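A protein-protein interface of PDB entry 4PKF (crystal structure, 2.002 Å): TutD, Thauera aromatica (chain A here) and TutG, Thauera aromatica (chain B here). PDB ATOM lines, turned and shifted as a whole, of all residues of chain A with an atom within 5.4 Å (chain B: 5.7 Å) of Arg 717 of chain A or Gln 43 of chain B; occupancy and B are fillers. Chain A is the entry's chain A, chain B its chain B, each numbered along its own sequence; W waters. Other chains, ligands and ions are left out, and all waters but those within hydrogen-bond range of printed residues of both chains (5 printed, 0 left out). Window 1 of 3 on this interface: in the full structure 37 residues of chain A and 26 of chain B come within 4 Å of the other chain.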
ATOM      1  N   GLN A 183       5.287 -16.550 -17.261  1.00  0.00           N
ATOM      2  CA  GLN A 183       4.894 -15.969 -15.979  1.00  0.00           C
ATOM      3  C   GLN A 183       6.040 -15.382 -15.170  1.00  0.00           C
ATOM      4  O   GLN A 183       5.804 -14.529 -14.296  1.00  0.00           O
ATOM      5  CB  GLN A 183       4.152 -17.015 -15.160  1.00  0.00           C
ATOM      6  CG  GLN A 183       2.793 -17.213 -15.805  1.00  0.00           C
ATOM      7  CD  GLN A 183       1.946 -18.214 -15.126  1.00  0.00           C
ATOM      8  OE1 GLN A 183       0.811 -18.448 -15.546  1.00  0.00           O
ATOM      9  NE2 GLN A 183       2.480 -18.852 -14.108  1.00  0.00           N
ATOM     10  N   VAL A 184       7.259 -15.829 -15.459  1.00  0.00           N
ATOM     11  CA  VAL A 184       8.459 -15.354 -14.751  1.00  0.00           C
ATOM     12  C   VAL A 184       8.273 -15.556 -13.237  1.00  0.00           C
ATOM     13  O   VAL A 184       8.394 -14.623 -12.424  1.00  0.00           O
ATOM     14  CB  VAL A 184       8.786 -13.863 -15.062  1.00  0.00           C
ATOM     15  CG1 VAL A 184      10.229 -13.506 -14.617  1.00  0.00           C
ATOM     16  CG2 VAL A 184       8.614 -13.562 -16.557  1.00  0.00           C
ATOM     17  N   SER A 185       7.983 -16.803 -12.875  1.00  0.00           N
ATOM     18  CA  SER A 185       7.827 -17.182 -11.481  1.00  0.00           C
ATOM     19  C   SER A 185       8.785 -18.315 -11.151  1.00  0.00           C
ATOM     20  O   SER A 185       9.541 -18.200 -10.179  1.00  0.00           O
ATOM     21  CB  SER A 185       6.375 -17.585 -11.190  1.00  0.00           C
ATOM     22  OG  SER A 185       5.968 -18.633 -12.047  1.00  0.00           O
ATOM     23  N   GLU A 382      11.333  -3.938 -14.891  1.00  0.00           N
ATOM     24  CA  GLU A 382      11.030  -4.350 -13.517  1.00  0.00           C
ATOM     25  C   GLU A 382      12.300  -4.721 -12.766  1.00  0.00           C
ATOM     26  O   GLU A 382      12.461  -4.376 -11.607  1.00  0.00           O
ATOM     27  CB  GLU A 382      10.070  -5.580 -13.487  1.00  0.00           C
ATOM     28  CG  GLU A 382       8.565  -5.298 -13.765  1.00  0.00           C
ATOM     29  CD  GLU A 382       7.678  -6.550 -13.564  1.00  0.00           C
ATOM     30  OE1 GLU A 382       8.197  -7.687 -13.717  1.00  0.00           O
ATOM     31  OE2 GLU A 382       6.477  -6.395 -13.201  1.00  0.00           O
ATOM     32  N   LYS A 518      10.581 -20.824  -6.144  1.00  0.00           N
ATOM     33  CA  LYS A 518       9.257 -21.132  -6.685  1.00  0.00           C
ATOM     34  C   LYS A 518       9.174 -22.612  -6.971  1.00  0.00           C
ATOM     35  O   LYS A 518       8.172 -23.251  -6.672  1.00  0.00           O
ATOM     36  CB  LYS A 518       8.956 -20.331  -7.960  1.00  0.00           C
ATOM     37  CG  LYS A 518       7.490 -20.384  -8.423  1.00  0.00           C
ATOM     38  CD  LYS A 518       6.520 -19.760  -7.329  1.00  0.00           C
ATOM     39  CE  LYS A 518       5.047 -19.800  -7.759  1.00  0.00           C
ATOM     40  NZ  LYS A 518       4.190 -19.098  -6.756  1.00  0.00           N
ATOM     41  N   GLU A 521       8.487 -24.205  -3.685  1.00  0.00           N
ATOM     42  CA  GLU A 521       7.085 -24.048  -3.328  1.00  0.00           C
ATOM     43  C   GLU A 521       6.187 -25.053  -4.064  1.00  0.00           C
ATOM     44  O   GLU A 521       5.379 -25.745  -3.422  1.00  0.00           O
ATOM     45  CB  GLU A 521       6.596 -22.620  -3.605  1.00  0.00           C
ATOM     46  CG  GLU A 521       5.158 -22.421  -3.154  1.00  0.00           C
ATOM     47  CD  GLU A 521       4.569 -21.053  -3.501  1.00  0.00           C
ATOM     48  OE1 GLU A 521       3.505 -20.700  -2.931  1.00  0.00           O
ATOM     49  OE2 GLU A 521       5.154 -20.333  -4.352  1.00  0.00           O
ATOM     50  N   ASP A 529       0.919 -24.370  -8.708  1.00  0.00           N
ATOM     51  CA  ASP A 529       1.144 -23.040  -8.132  1.00  0.00           C
ATOM     52  C   ASP A 529      -0.180 -22.512  -7.650  1.00  0.00           C
ATOM     53  O   ASP A 529      -0.944 -21.973  -8.460  1.00  0.00           O
ATOM     54  CB  ASP A 529       1.762 -22.079  -9.175  1.00  0.00           C
ATOM     55  CG  ASP A 529       1.732 -20.611  -8.733  1.00  0.00           C
ATOM     56  OD1 ASP A 529       1.706 -20.350  -7.506  1.00  0.00           O
ATOM     57  OD2 ASP A 529       1.721 -19.724  -9.631  1.00  0.00           O
ATOM     58  N   SER A 531      -0.529 -20.237  -5.256  1.00  0.00           N
ATOM     59  CA  SER A 531      -0.393 -18.924  -4.613  1.00  0.00           C
ATOM     60  C   SER A 531      -0.302 -17.740  -5.575  1.00  0.00           C
ATOM     61  O   SER A 531      -0.802 -16.650  -5.248  1.00  0.00           O
ATOM     62  CB  SER A 531       0.837 -18.909  -3.689  1.00  0.00           C
ATOM     63  OG  SER A 531       2.005 -19.204  -4.446  1.00  0.00           O
ATOM     64  N   TYR A 532       0.328 -17.920  -6.742  1.00  0.00           N
ATOM     65  CA  TYR A 532       0.421 -16.808  -7.693  1.00  0.00           C
ATOM     66  C   TYR A 532      -0.530 -17.024  -8.852  1.00  0.00           C
ATOM     67  O   TYR A 532      -1.495 -16.281  -9.013  1.00  0.00           O
ATOM     68  CB  TYR A 532       1.871 -16.617  -8.192  1.00  0.00           C
ATOM     69  CG  TYR A 532       2.028 -15.507  -9.227  1.00  0.00           C
ATOM     70  CD1 TYR A 532       1.632 -14.205  -8.944  1.00  0.00           C
ATOM     71  CD2 TYR A 532       2.566 -15.770 -10.481  1.00  0.00           C
ATOM     72  CE1 TYR A 532       1.755 -13.217  -9.874  1.00  0.00           C
ATOM     73  CE2 TYR A 532       2.706 -14.769 -11.435  1.00  0.00           C
ATOM     74  CZ  TYR A 532       2.294 -13.505 -11.129  1.00  0.00           C
ATOM     75  OH  TYR A 532       2.435 -12.511 -12.050  1.00  0.00           O
ATOM     76  N   LEU A 710      15.454  -9.542  -9.803  1.00  0.00           N
ATOM     77  CA  LEU A 710      14.528 -10.672  -9.867  1.00  0.00           C
ATOM     78  C   LEU A 710      14.241 -11.234  -8.470  1.00  0.00           C
ATOM     79  O   LEU A 710      13.181 -11.809  -8.254  1.00  0.00           O
ATOM     80  CB  LEU A 710      15.082 -11.754 -10.799  1.00  0.00           C
ATOM     81  CG  LEU A 710      14.713 -11.501 -12.288  1.00  0.00           C
ATOM     82  CD1 LEU A 710      15.628 -12.282 -13.245  1.00  0.00           C
ATOM     83  CD2 LEU A 710      13.207 -11.880 -12.555  1.00  0.00           C
ATOM     84  N   MET A 712      13.519  -9.631  -6.006  1.00  0.00           N
ATOM     85  CA  MET A 712      12.332  -8.878  -5.610  1.00  0.00           C
ATOM     86  C   MET A 712      11.080  -9.316  -6.374  1.00  0.00           C
ATOM     87  O   MET A 712      10.023  -9.549  -5.782  1.00  0.00           O
ATOM     88  CB  MET A 712      12.589  -7.376  -5.859  1.00  0.00           C
ATOM     89  CG  MET A 712      13.789  -6.788  -5.034  1.00  0.00           C
ATOM     90  SD  MET A 712      14.154  -5.152  -5.762  1.00  0.00           S
ATOM     91  CE  MET A 712      15.718  -4.699  -4.977  1.00  0.00           C
ATOM     92  N   GLU A 713      11.181  -9.396  -7.705  1.00  0.00           N
ATOM     93  CA  GLU A 713       9.985  -9.679  -8.494  1.00  0.00           C
ATOM     94  C   GLU A 713       9.512 -11.100  -8.274  1.00  0.00           C
ATOM     95  O   GLU A 713       8.324 -11.346  -8.121  1.00  0.00           O
ATOM     96  CB  GLU A 713      10.219  -9.443 -10.003  1.00  0.00           C
ATOM     97  CG  GLU A 713      10.432  -7.975 -10.378  1.00  0.00           C
ATOM     98  CD  GLU A 713       9.218  -7.076 -10.120  1.00  0.00           C
ATOM     99  OE1 GLU A 713       8.109  -7.574  -9.826  1.00  0.00           O
ATOM    100  OE2 GLU A 713       9.386  -5.843 -10.213  1.00  0.00           O
ATOM    101  N   VAL A 714      10.446 -12.039  -8.258  1.00  0.00           N
ATOM    102  CA  VAL A 714      10.073 -13.433  -8.024  1.00  0.00           C
ATOM    103  C   VAL A 714       9.561 -13.603  -6.580  1.00  0.00           C
ATOM    104  O   VAL A 714       8.638 -14.386  -6.362  1.00  0.00           O
ATOM    105  CB  VAL A 714      11.257 -14.397  -8.316  1.00  0.00           C
ATOM    106  CG1 VAL A 714      10.930 -15.818  -7.942  1.00  0.00           C
ATOM    107  CG2 VAL A 714      11.635 -14.298  -9.793  1.00  0.00           C
ATOM    108  N   GLY A 715      10.154 -12.880  -5.618  1.00  0.00           N
ATOM    109  CA  GLY A 715       9.676 -12.898  -4.226  1.00  0.00           C
ATOM    110  C   GLY A 715       8.201 -12.570  -4.184  1.00  0.00           C
ATOM    111  O   GLY A 715       7.378 -13.260  -3.543  1.00  0.00           O
ATOM    112  N   SER A 716       7.839 -11.514  -4.896  1.00  0.00           N
ATOM    113  CA  SER A 716       6.450 -11.070  -4.936  1.00  0.00           C
ATOM    114  C   SER A 716       5.503 -12.067  -5.636  1.00  0.00           C
ATOM    115  O   SER A 716       4.271 -11.958  -5.492  1.00  0.00           O
ATOM    116  CB  SER A 716       6.381  -9.708  -5.627  1.00  0.00           C
ATOM    117  OG  SER A 716       6.545  -9.814  -7.028  1.00  0.00           O
ATOM    118  N   ARG A 717       6.057 -13.044  -6.372  1.00  0.00           N
ATOM    119  CA  ARG A 717       5.236 -14.039  -7.075  1.00  0.00           C
ATOM    120  C   ARG A 717       5.334 -15.409  -6.397  1.00  0.00           C
ATOM    121  O   ARG A 717       4.872 -16.416  -6.931  1.00  0.00           O
ATOM    122  CB  ARG A 717       5.677 -14.167  -8.557  1.00  0.00           C
ATOM    123  CG  ARG A 717       5.474 -12.907  -9.402  1.00  0.00           C
ATOM    124  CD  ARG A 717       5.996 -13.007 -10.887  1.00  0.00           C
ATOM    125  NE  ARG A 717       5.921 -11.674 -11.489  1.00  0.00           N
ATOM    126  CZ  ARG A 717       6.920 -11.051 -12.088  1.00  0.00           C
ATOM    127  NH1 ARG A 717       6.731  -9.820 -12.546  1.00  0.00           N
ATOM    128  NH2 ARG A 717       8.084 -11.662 -12.256  1.00  0.00           N
ATOM    129  N   THR A 718       6.038 -15.453  -5.280  1.00  0.00           N
ATOM    130  CA  THR A 718       6.250 -16.693  -4.560  1.00  0.00           C
ATOM    131  C   THR A 718       5.486 -16.691  -3.208  1.00  0.00           C
ATOM    132  O   THR A 718       5.515 -15.702  -2.464  1.00  0.00           O
ATOM    133  CB  THR A 718       7.749 -16.918  -4.331  1.00  0.00           C
ATOM    134  OG1 THR A 718       8.392 -17.026  -5.605  1.00  0.00           O
ATOM    135  CG2 THR A 718       7.980 -18.218  -3.571  1.00  0.00           C
ATOM    136  N   GLY A 719       4.808 -17.799  -2.907  1.00  0.00           N
ATOM    137  CA  GLY A 719       4.045 -17.892  -1.659  1.00  0.00           C
ATOM    138  C   GLY A 719       4.931 -18.023  -0.445  1.00  0.00           C
ATOM    139  O   GLY A 719       6.164 -17.989  -0.531  1.00  0.00           O
ATOM    140  N   GLY A 728       4.930 -13.303  -0.907  1.00  0.00           N
ATOM    141  CA  GLY A 728       5.236 -12.014  -1.502  1.00  0.00           C
ATOM    142  C   GLY A 728       6.409 -11.231  -0.923  1.00  0.00           C
ATOM    143  O   GLY A 728       6.696 -10.101  -1.355  1.00  0.00           O
ATOM    144  N   TRP B  31      -4.228  -1.135  -8.267  1.00  0.00           N
ATOM    145  CA  TRP B  31      -3.496  -2.259  -7.703  1.00  0.00           C
ATOM    146  C   TRP B  31      -2.886  -3.157  -8.778  1.00  0.00           C
ATOM    147  O   TRP B  31      -1.979  -3.939  -8.466  1.00  0.00           O
ATOM    148  CB  TRP B  31      -4.406  -3.087  -6.803  1.00  0.00           C
ATOM    149  CG  TRP B  31      -4.883  -2.312  -5.614  1.00  0.00           C
ATOM    150  CD1 TRP B  31      -6.178  -1.998  -5.290  1.00  0.00           C
ATOM    151  CD2 TRP B  31      -4.057  -1.737  -4.583  1.00  0.00           C
ATOM    152  NE1 TRP B  31      -6.199  -1.254  -4.121  1.00  0.00           N
ATOM    153  CE2 TRP B  31      -4.916  -1.093  -3.666  1.00  0.00           C
ATOM    154  CE3 TRP B  31      -2.678  -1.718  -4.345  1.00  0.00           C
ATOM    155  CZ2 TRP B  31      -4.440  -0.428  -2.546  1.00  0.00           C
ATOM    156  CZ3 TRP B  31      -2.203  -1.062  -3.232  1.00  0.00           C
ATOM    157  CH2 TRP B  31      -3.087  -0.436  -2.331  1.00  0.00           C
ATOM    158  N   GLN B  32      -3.402  -3.045 -10.012  1.00  0.00           N
ATOM    159  CA  GLN B  32      -2.929  -3.835 -11.159  1.00  0.00           C
ATOM    160  C   GLN B  32      -1.681  -3.226 -11.794  1.00  0.00           C
ATOM    161  O   GLN B  32      -1.570  -2.010 -11.901  1.00  0.00           O
ATOM    162  CB  GLN B  32      -4.015  -3.952 -12.237  1.00  0.00           C
ATOM    163  CG  GLN B  32      -3.759  -4.982 -13.346  1.00  0.00           C
ATOM    164  CD  GLN B  32      -2.983  -4.442 -14.577  1.00  0.00           C
ATOM    165  OE1 GLN B  32      -2.550  -5.227 -15.410  1.00  0.00           O
ATOM    166  NE2 GLN B  32      -2.827  -3.124 -14.693  1.00  0.00           N
ATOM    167  N   THR B  33      -0.747  -4.082 -12.202  1.00  0.00           N
ATOM    168  CA  THR B  33       0.350  -3.675 -13.108  1.00  0.00           C
ATOM    169  C   THR B  33       0.458  -4.820 -14.149  1.00  0.00           C
ATOM    170  O   THR B  33       0.167  -5.996 -13.831  1.00  0.00           O
ATOM    171  CB  THR B  33       1.681  -3.389 -12.320  1.00  0.00           C
ATOM    172  OG1 THR B  33       2.647  -2.815 -13.190  1.00  0.00           O
ATOM    173  CG2 THR B  33       2.267  -4.642 -11.729  1.00  0.00           C
ATOM    174  N   PRO B  34       0.766  -4.484 -15.413  1.00  0.00           N
ATOM    175  CA  PRO B  34       0.744  -5.533 -16.448  1.00  0.00           C
ATOM    176  C   PRO B  34       1.758  -6.665 -16.179  1.00  0.00           C
ATOM    177  O   PRO B  34       2.784  -6.463 -15.543  1.00  0.00           O
ATOM    178  CB  PRO B  34       1.108  -4.767 -17.735  1.00  0.00           C
ATOM    179  CG  PRO B  34       0.721  -3.344 -17.464  1.00  0.00           C
ATOM    180  CD  PRO B  34       0.975  -3.137 -15.983  1.00  0.00           C
ATOM    181  N   ASP B  35       1.421  -7.859 -16.646  1.00  0.00           N
ATOM    182  CA  ASP B  35       2.305  -9.024 -16.659  1.00  0.00           C
ATOM    183  C   ASP B  35       3.669  -8.703 -17.323  1.00  0.00           C
ATOM    184  O   ASP B  35       3.737  -7.900 -18.250  1.00  0.00           O
ATOM    185  CB  ASP B  35       1.555 -10.145 -17.402  1.00  0.00           C
ATOM    186  CG  ASP B  35       2.333 -11.433 -17.535  1.00  0.00           C
ATOM    187  OD1 ASP B  35       3.155 -11.532 -18.462  1.00  0.00           O
ATOM    188  OD2 ASP B  35       2.072 -12.391 -16.765  1.00  0.00           O
ATOM    189  N   PRO B  36       4.765  -9.299 -16.825  1.00  0.00           N
ATOM    190  CA  PRO B  36       6.086  -8.953 -17.355  1.00  0.00           C
ATOM    191  C   PRO B  36       6.318  -9.331 -18.828  1.00  0.00           C
ATOM    192  O   PRO B  36       7.166  -8.710 -19.482  1.00  0.00           O
ATOM    193  CB  PRO B  36       7.037  -9.744 -16.446  1.00  0.00           C
ATOM    194  CG  PRO B  36       6.199 -10.859 -15.897  1.00  0.00           C
ATOM    195  CD  PRO B  36       4.863 -10.218 -15.679  1.00  0.00           C
ATOM    196  N   ARG B  41      -2.150 -10.030 -19.956  1.00  0.00           N
ATOM    197  CA  ARG B  41      -2.238 -10.514 -18.594  1.00  0.00           C
ATOM    198  C   ARG B  41      -1.872  -9.425 -17.596  1.00  0.00           C
ATOM    199  O   ARG B  41      -1.311  -8.399 -17.960  1.00  0.00           O
ATOM    200  CB  ARG B  41      -1.317 -11.713 -18.379  1.00  0.00           C
ATOM    201  CG  ARG B  41      -1.259 -12.676 -19.556  1.00  0.00           C
ATOM    202  CD  ARG B  41      -2.520 -13.441 -19.706  1.00  0.00           C
ATOM    203  NE  ARG B  41      -2.298 -14.606 -20.561  1.00  0.00           N
ATOM    204  CZ  ARG B  41      -3.161 -15.605 -20.713  1.00  0.00           C
ATOM    205  NH1 ARG B  41      -2.869 -16.620 -21.517  1.00  0.00           N
ATOM    206  NH2 ARG B  41      -4.316 -15.584 -20.075  1.00  0.00           N
ATOM    207  N   GLY B  42      -2.181  -9.663 -16.328  1.00  0.00           N
ATOM    208  CA  GLY B  42      -1.895  -8.675 -15.308  1.00  0.00           C
ATOM    209  C   GLY B  42      -1.392  -9.238 -13.992  1.00  0.00           C
ATOM    210  O   GLY B  42      -1.411 -10.440 -13.785  1.00  0.00           O
ATOM    211  N   GLN B  43      -0.927  -8.336 -13.112  1.00  0.00           N
ATOM    212  CA  GLN B  43      -0.509  -8.655 -11.760  1.00  0.00           C
ATOM    213  C   GLN B  43      -1.334  -7.816 -10.784  1.00  0.00           C
ATOM    214  O   GLN B  43      -1.255  -6.586 -10.815  1.00  0.00           O
ATOM    215  CB  GLN B  43       0.984  -8.355 -11.524  1.00  0.00           C
ATOM    216  CG  GLN B  43       1.944  -8.983 -12.567  1.00  0.00           C
ATOM    217  CD  GLN B  43       3.388  -8.569 -12.345  1.00  0.00           C
ATOM    218  OE1 GLN B  43       4.040  -9.015 -11.387  1.00  0.00           O
ATOM    219  NE2 GLN B  43       3.896  -7.697 -13.229  1.00  0.00           N
ATOM    220  N   CYS B  44      -2.097  -8.478  -9.913  1.00  0.00           N
ATOM    221  CA  CYS B  44      -2.839  -7.781  -8.857  1.00  0.00           C
ATOM    222  C   CYS B  44      -1.950  -7.660  -7.641  1.00  0.00           C
ATOM    223  O   CYS B  44      -1.461  -8.669  -7.120  1.00  0.00           O
ATOM    224  CB  CYS B  44      -4.140  -8.517  -8.494  1.00  0.00           C
ATOM    225  SG  CYS B  44      -4.936  -7.833  -6.973  1.00  0.00           S
ATOM    226  N   THR B  45      -1.716  -6.432  -7.183  1.00  0.00           N
ATOM    227  CA  THR B  45      -0.792  -6.234  -6.078  1.00  0.00           C
ATOM    228  C   THR B  45      -1.558  -5.853  -4.804  1.00  0.00           C
ATOM    229  O   THR B  45      -0.963  -5.367  -3.849  1.00  0.00           O
ATOM    230  CB  THR B  45       0.265  -5.144  -6.392  1.00  0.00           C
ATOM    231  OG1 THR B  45      -0.377  -3.873  -6.507  1.00  0.00           O
ATOM    232  CG2 THR B  45       1.003  -5.436  -7.752  1.00  0.00           C
ATOM    233  N   VAL B  54       4.385  -8.101  -0.745  1.00  0.00           N
ATOM    234  CA  VAL B  54       3.401  -7.742  -1.758  1.00  0.00           C
ATOM    235  C   VAL B  54       3.053  -9.045  -2.465  1.00  0.00           C
ATOM    236  O   VAL B  54       3.742  -9.490  -3.403  1.00  0.00           O
ATOM    237  CB  VAL B  54       3.930  -6.683  -2.748  1.00  0.00           C
ATOM    238  CG1 VAL B  54       2.878  -6.380  -3.811  1.00  0.00           C
ATOM    239  CG2 VAL B  54       4.331  -5.380  -1.974  1.00  0.00           C
ATOM    240  N   LYS B  56       1.398 -11.029  -4.761  1.00  0.00           N
ATOM    241  CA  LYS B  56       0.694 -10.807  -6.028  1.00  0.00           C
ATOM    242  C   LYS B  56      -0.233 -11.949  -6.439  1.00  0.00           C
ATOM    243  O   LYS B  56      -0.036 -13.085  -6.034  1.00  0.00           O
ATOM    244  CB  LYS B  56       1.704 -10.577  -7.143  1.00  0.00           C
ATOM    245  CG  LYS B  56       2.437  -9.246  -7.080  1.00  0.00           C
ATOM    246  CD  LYS B  56       3.532  -9.220  -8.121  1.00  0.00           C
ATOM    247  CE  LYS B  56       4.210  -7.837  -8.189  1.00  0.00           C
ATOM    248  NZ  LYS B  56       5.307  -7.827  -9.243  1.00  0.00           N
ATOM    249  N   ARG B  57      -1.231 -11.633  -7.267  1.00  0.00           N
ATOM    250  CA  ARG B  57      -2.051 -12.676  -7.888  1.00  0.00           C
ATOM    251  C   ARG B  57      -2.022 -12.473  -9.380  1.00  0.00           C
ATOM    252  O   ARG B  57      -2.159 -11.337  -9.871  1.00  0.00           O
ATOM    253  CB  ARG B  57      -3.501 -12.645  -7.389  1.00  0.00           C
ATOM    254  CG  ARG B  57      -3.704 -13.129  -5.972  1.00  0.00           C
ATOM    255  CD  ARG B  57      -3.231 -14.575  -5.849  1.00  0.00           C
ATOM    256  NE  ARG B  57      -3.427 -15.135  -4.509  1.00  0.00           N
ATOM    257  CZ  ARG B  57      -2.714 -14.819  -3.427  1.00  0.00           C
ATOM    258  NH1 ARG B  57      -2.988 -15.399  -2.264  1.00  0.00           N
ATOM    259  NH2 ARG B  57      -1.735 -13.927  -3.499  1.00  0.00           N
ATOM    260  N   TRP B  58      -1.838 -13.561 -10.120  1.00  0.00           N
ATOM    261  CA  TRP B  58      -1.771 -13.458 -11.577  1.00  0.00           C
ATOM    262  C   TRP B  58      -3.163 -13.276 -12.199  1.00  0.00           C
ATOM    263  O   TRP B  58      -4.113 -13.958 -11.810  1.00  0.00           O
ATOM    264  CB  TRP B  58      -1.076 -14.705 -12.166  1.00  0.00           C
ATOM    265  CG  TRP B  58      -0.821 -14.617 -13.641  1.00  0.00           C
ATOM    266  CD1 TRP B  58      -0.011 -13.701 -14.298  1.00  0.00           C
ATOM    267  CD2 TRP B  58      -1.367 -15.459 -14.662  1.00  0.00           C
ATOM    268  NE1 TRP B  58      -0.021 -13.942 -15.635  1.00  0.00           N
ATOM    269  CE2 TRP B  58      -0.838 -15.014 -15.894  1.00  0.00           C
ATOM    270  CE3 TRP B  58      -2.213 -16.575 -14.652  1.00  0.00           C
ATOM    271  CZ2 TRP B  58      -1.145 -15.636 -17.110  1.00  0.00           C
ATOM    272  CZ3 TRP B  58      -2.534 -17.176 -15.838  1.00  0.00           C
ATOM    273  CH2 TRP B  58      -1.990 -16.715 -17.066  1.00  0.00           C
ATOM    274  N   LEU B  59      -3.278 -12.354 -13.145  1.00  0.00           N
ATOM    275  CA  LEU B  59      -4.558 -12.085 -13.785  1.00  0.00           C
ATOM    276  C   LEU B  59      -4.530 -12.551 -15.251  1.00  0.00           C
ATOM    277  O   LEU B  59      -3.784 -11.977 -16.061  1.00  0.00           O
ATOM    278  CB  LEU B  59      -4.879 -10.582 -13.708  1.00  0.00           C
ATOM    279  CG  LEU B  59      -4.886  -9.902 -12.322  1.00  0.00           C
ATOM    280  CD1 LEU B  59      -5.028  -8.397 -12.480  1.00  0.00           C
ATOM    281  CD2 LEU B  59      -6.021 -10.485 -11.438  1.00  0.00           C
ATOM    282  N   VAL B  62      -7.449  -8.969 -17.947  1.00  0.00           N
ATOM    283  CA  VAL B  62      -7.653  -7.736 -17.210  1.00  0.00           C
ATOM    284  C   VAL B  62      -8.821  -6.883 -17.716  1.00  0.00           C
ATOM    285  O   VAL B  62      -9.046  -5.788 -17.208  1.00  0.00           O
ATOM    286  CB  VAL B  62      -6.369  -6.894 -17.233  1.00  0.00           C
ATOM    287  CG1 VAL B  62      -5.266  -7.618 -16.453  1.00  0.00           C
ATOM    288  CG2 VAL B  62      -5.940  -6.654 -18.675  1.00  0.00           C
HETATM  289  O   HOH W   1       4.890  -4.036 -14.066  1.00  0.00           O
HETATM  290  O   HOH W   2      -4.094 -16.317 -10.236  1.00  0.00           O
HETATM  291  O   HOH W   3       2.325 -14.194  -5.371  1.00  0.00           O
HETATM  292  O   HOH W   4       3.524 -13.022 -14.377  1.00  0.00           O
HETATM  293  O   HOH W   5       5.889  -5.263 -10.375  1.00  0.00           O
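Of the 19 printed residues of chain A, 9 touch a printed residue of chain B. Hydrophobic or aromatic side chains of chain A that line the printed part of chain B: Val 184 and Tyr 532. Among the printed residues, 16 pairs touch across the chains. Among the printed residues, Asp or Glu carboxylates within 4 Å of a Lys or Arg side-chain nitrogen of the other chain: Glu 713 of chain A with Lys 56 of chain B (2.9 Å).
CZ3 of Trp 58 of chain B touches OE1 of Gln 183 of chain A, 3.6 Å away. Val 184 of chain A touches Pro 36 of chain B. OE1 of Glu 382 of chain A touches CB of Pro 36 of chain B, at 3.6 Å. Lys 56 of chain B touches Ser 531 of chain A. Gln 43 of chain B touches Tyr 532 of chain A. CD1 of Tyr 532 of chain A touches O of Lys 56 of chain B, 3.5 Å away. Tyr 532 of chain A touches Arg 57 of chain B (O to CA, 3.8 Å). NH1 of Arg 717 of chain A touches CG of Pro 36 of chain B, at 3.5 Å.
The side-chain carboxylate of Glu 382 of chain A lies within hydrogen-bond range of the side-chain amide nitrogen of Gln 43 of chain B (2.9 Å). O of Ser 531 of chain A sits at hydrogen-bond distance from NE of Arg 57 of chain B, at 3.1 Å. N of Trp 58 of chain B is in hydrogen-bond range of O of Tyr 532 of chain A (3.0 Å). The side-chain carboxylate (OE1) of Glu 713 of chain A lies within salt-bridge range of the side-chain amino group (NZ) of Lys 56 of chain B, at 2.9 Å. The backbone carbonyl oxygen (O) of Ser 716 of chain A sits at hydrogen-bond distance from the backbone NH (N) of Lys 56 of chain B, 3.1 Å away. OE1 of Gln 43 of chain B is in hydrogen-bond range of NH1 of Arg 717 of chain A (3.0 Å). The backbone carbonyl oxygen (O) of Gly 728 of chain A lies within hydrogen-bond range of the backbone NH (N) of Val 54 of chain B, at 3.1 Å. The backbone carbonyl oxygen (O) of Val 54 of chain B sits close to the backbone carbonyl oxygen (O) of Ser 716 of chain A, 3.3 Å away.
Of chain B, only Pro 36 and Gln 43 come within 4 Å of Arg 717 of chain A. Gln 43 of chain B touches three residues of chain A. Printed residues of chain A within 4 Å of Lys 56 of chain B: Ser 531 (3.7 Å), Tyr 532 (3.5 Å), Glu 713 (2.9 Å) and Ser 716 (3.1 Å). Printed residues of chain B within 4 Å of Ser 716 of chain A: Val 54 (3.3 Å) and Lys 56 (3.1 Å). The nearest residue of chain A that does not touch Gln 43 of chain B is Glu 713 of chain A (4.6 Å).
OE1 of Glu 382 of chain A is in salt-bridge range of NH1 of Arg 717 of chain A. The side-chain carboxylate (OD1) of Asp 529 of chain A lies within hydrogen-bond range of the backbone NH (N) of Tyr 532 of chain A (2.9 Å). The side-chain hydroxyl (OG) of Ser 531 of chain A lies within hydrogen-bond range of the backbone NH (N) of Gly 719 of chain A, at 3.5 Å. The backbone carbonyl oxygen of Pro 34 of chain B sits at hydrogen-bond distance from the side-chain amide nitrogen of Gln 43 of chain B. NE1 of Trp 58 of chain B sits at hydrogen-bond distance from OD2 of Asp 35 of chain B (2.8 Å). The backbone carbonyl oxygen (O) of Arg 57 of chain B is in hydrogen-bond range of the backbone NH (N) of Cys 44 of chain B, at 2.9 Å.
Water W4 lies within hydrogen-bond range of the side-chain hydroxyl (OH) of Tyr 532 of chain A (2.6 Å), the backbone carbonyl oxygen (O) of Gln 183 of chain A (2.7 Å) and the side-chain carboxylate (OD2) of Asp 35 of chain B (2.9 Å). Water W3 lies within hydrogen-bond range of the backbone carbonyl oxygen of Lys 56 of chain B (2.7 Å) and the backbone carbonyl oxygen of Ser 716 of chain A (3.0 Å). Water W1 bridges OG1 of Thr 33 of chain B (2.7 Å) and OE2 of Glu 382 of chain A (3.0 Å). Water W2 lies within hydrogen-bond range of the backbone carbonyl oxygen (O) of Trp 58 of chain B (2.8 Å) and the backbone carbonyl oxygen (O) of Tyr 532 of chain A (2.9 Å). Water W5 lies within hydrogen-bond range of NZ of Lys 56 of chain B (2.9 Å), OE2 of Glu 382 of chain A (3.1 Å) and OE1 of Glu 713 of chain A (3.3 Å).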
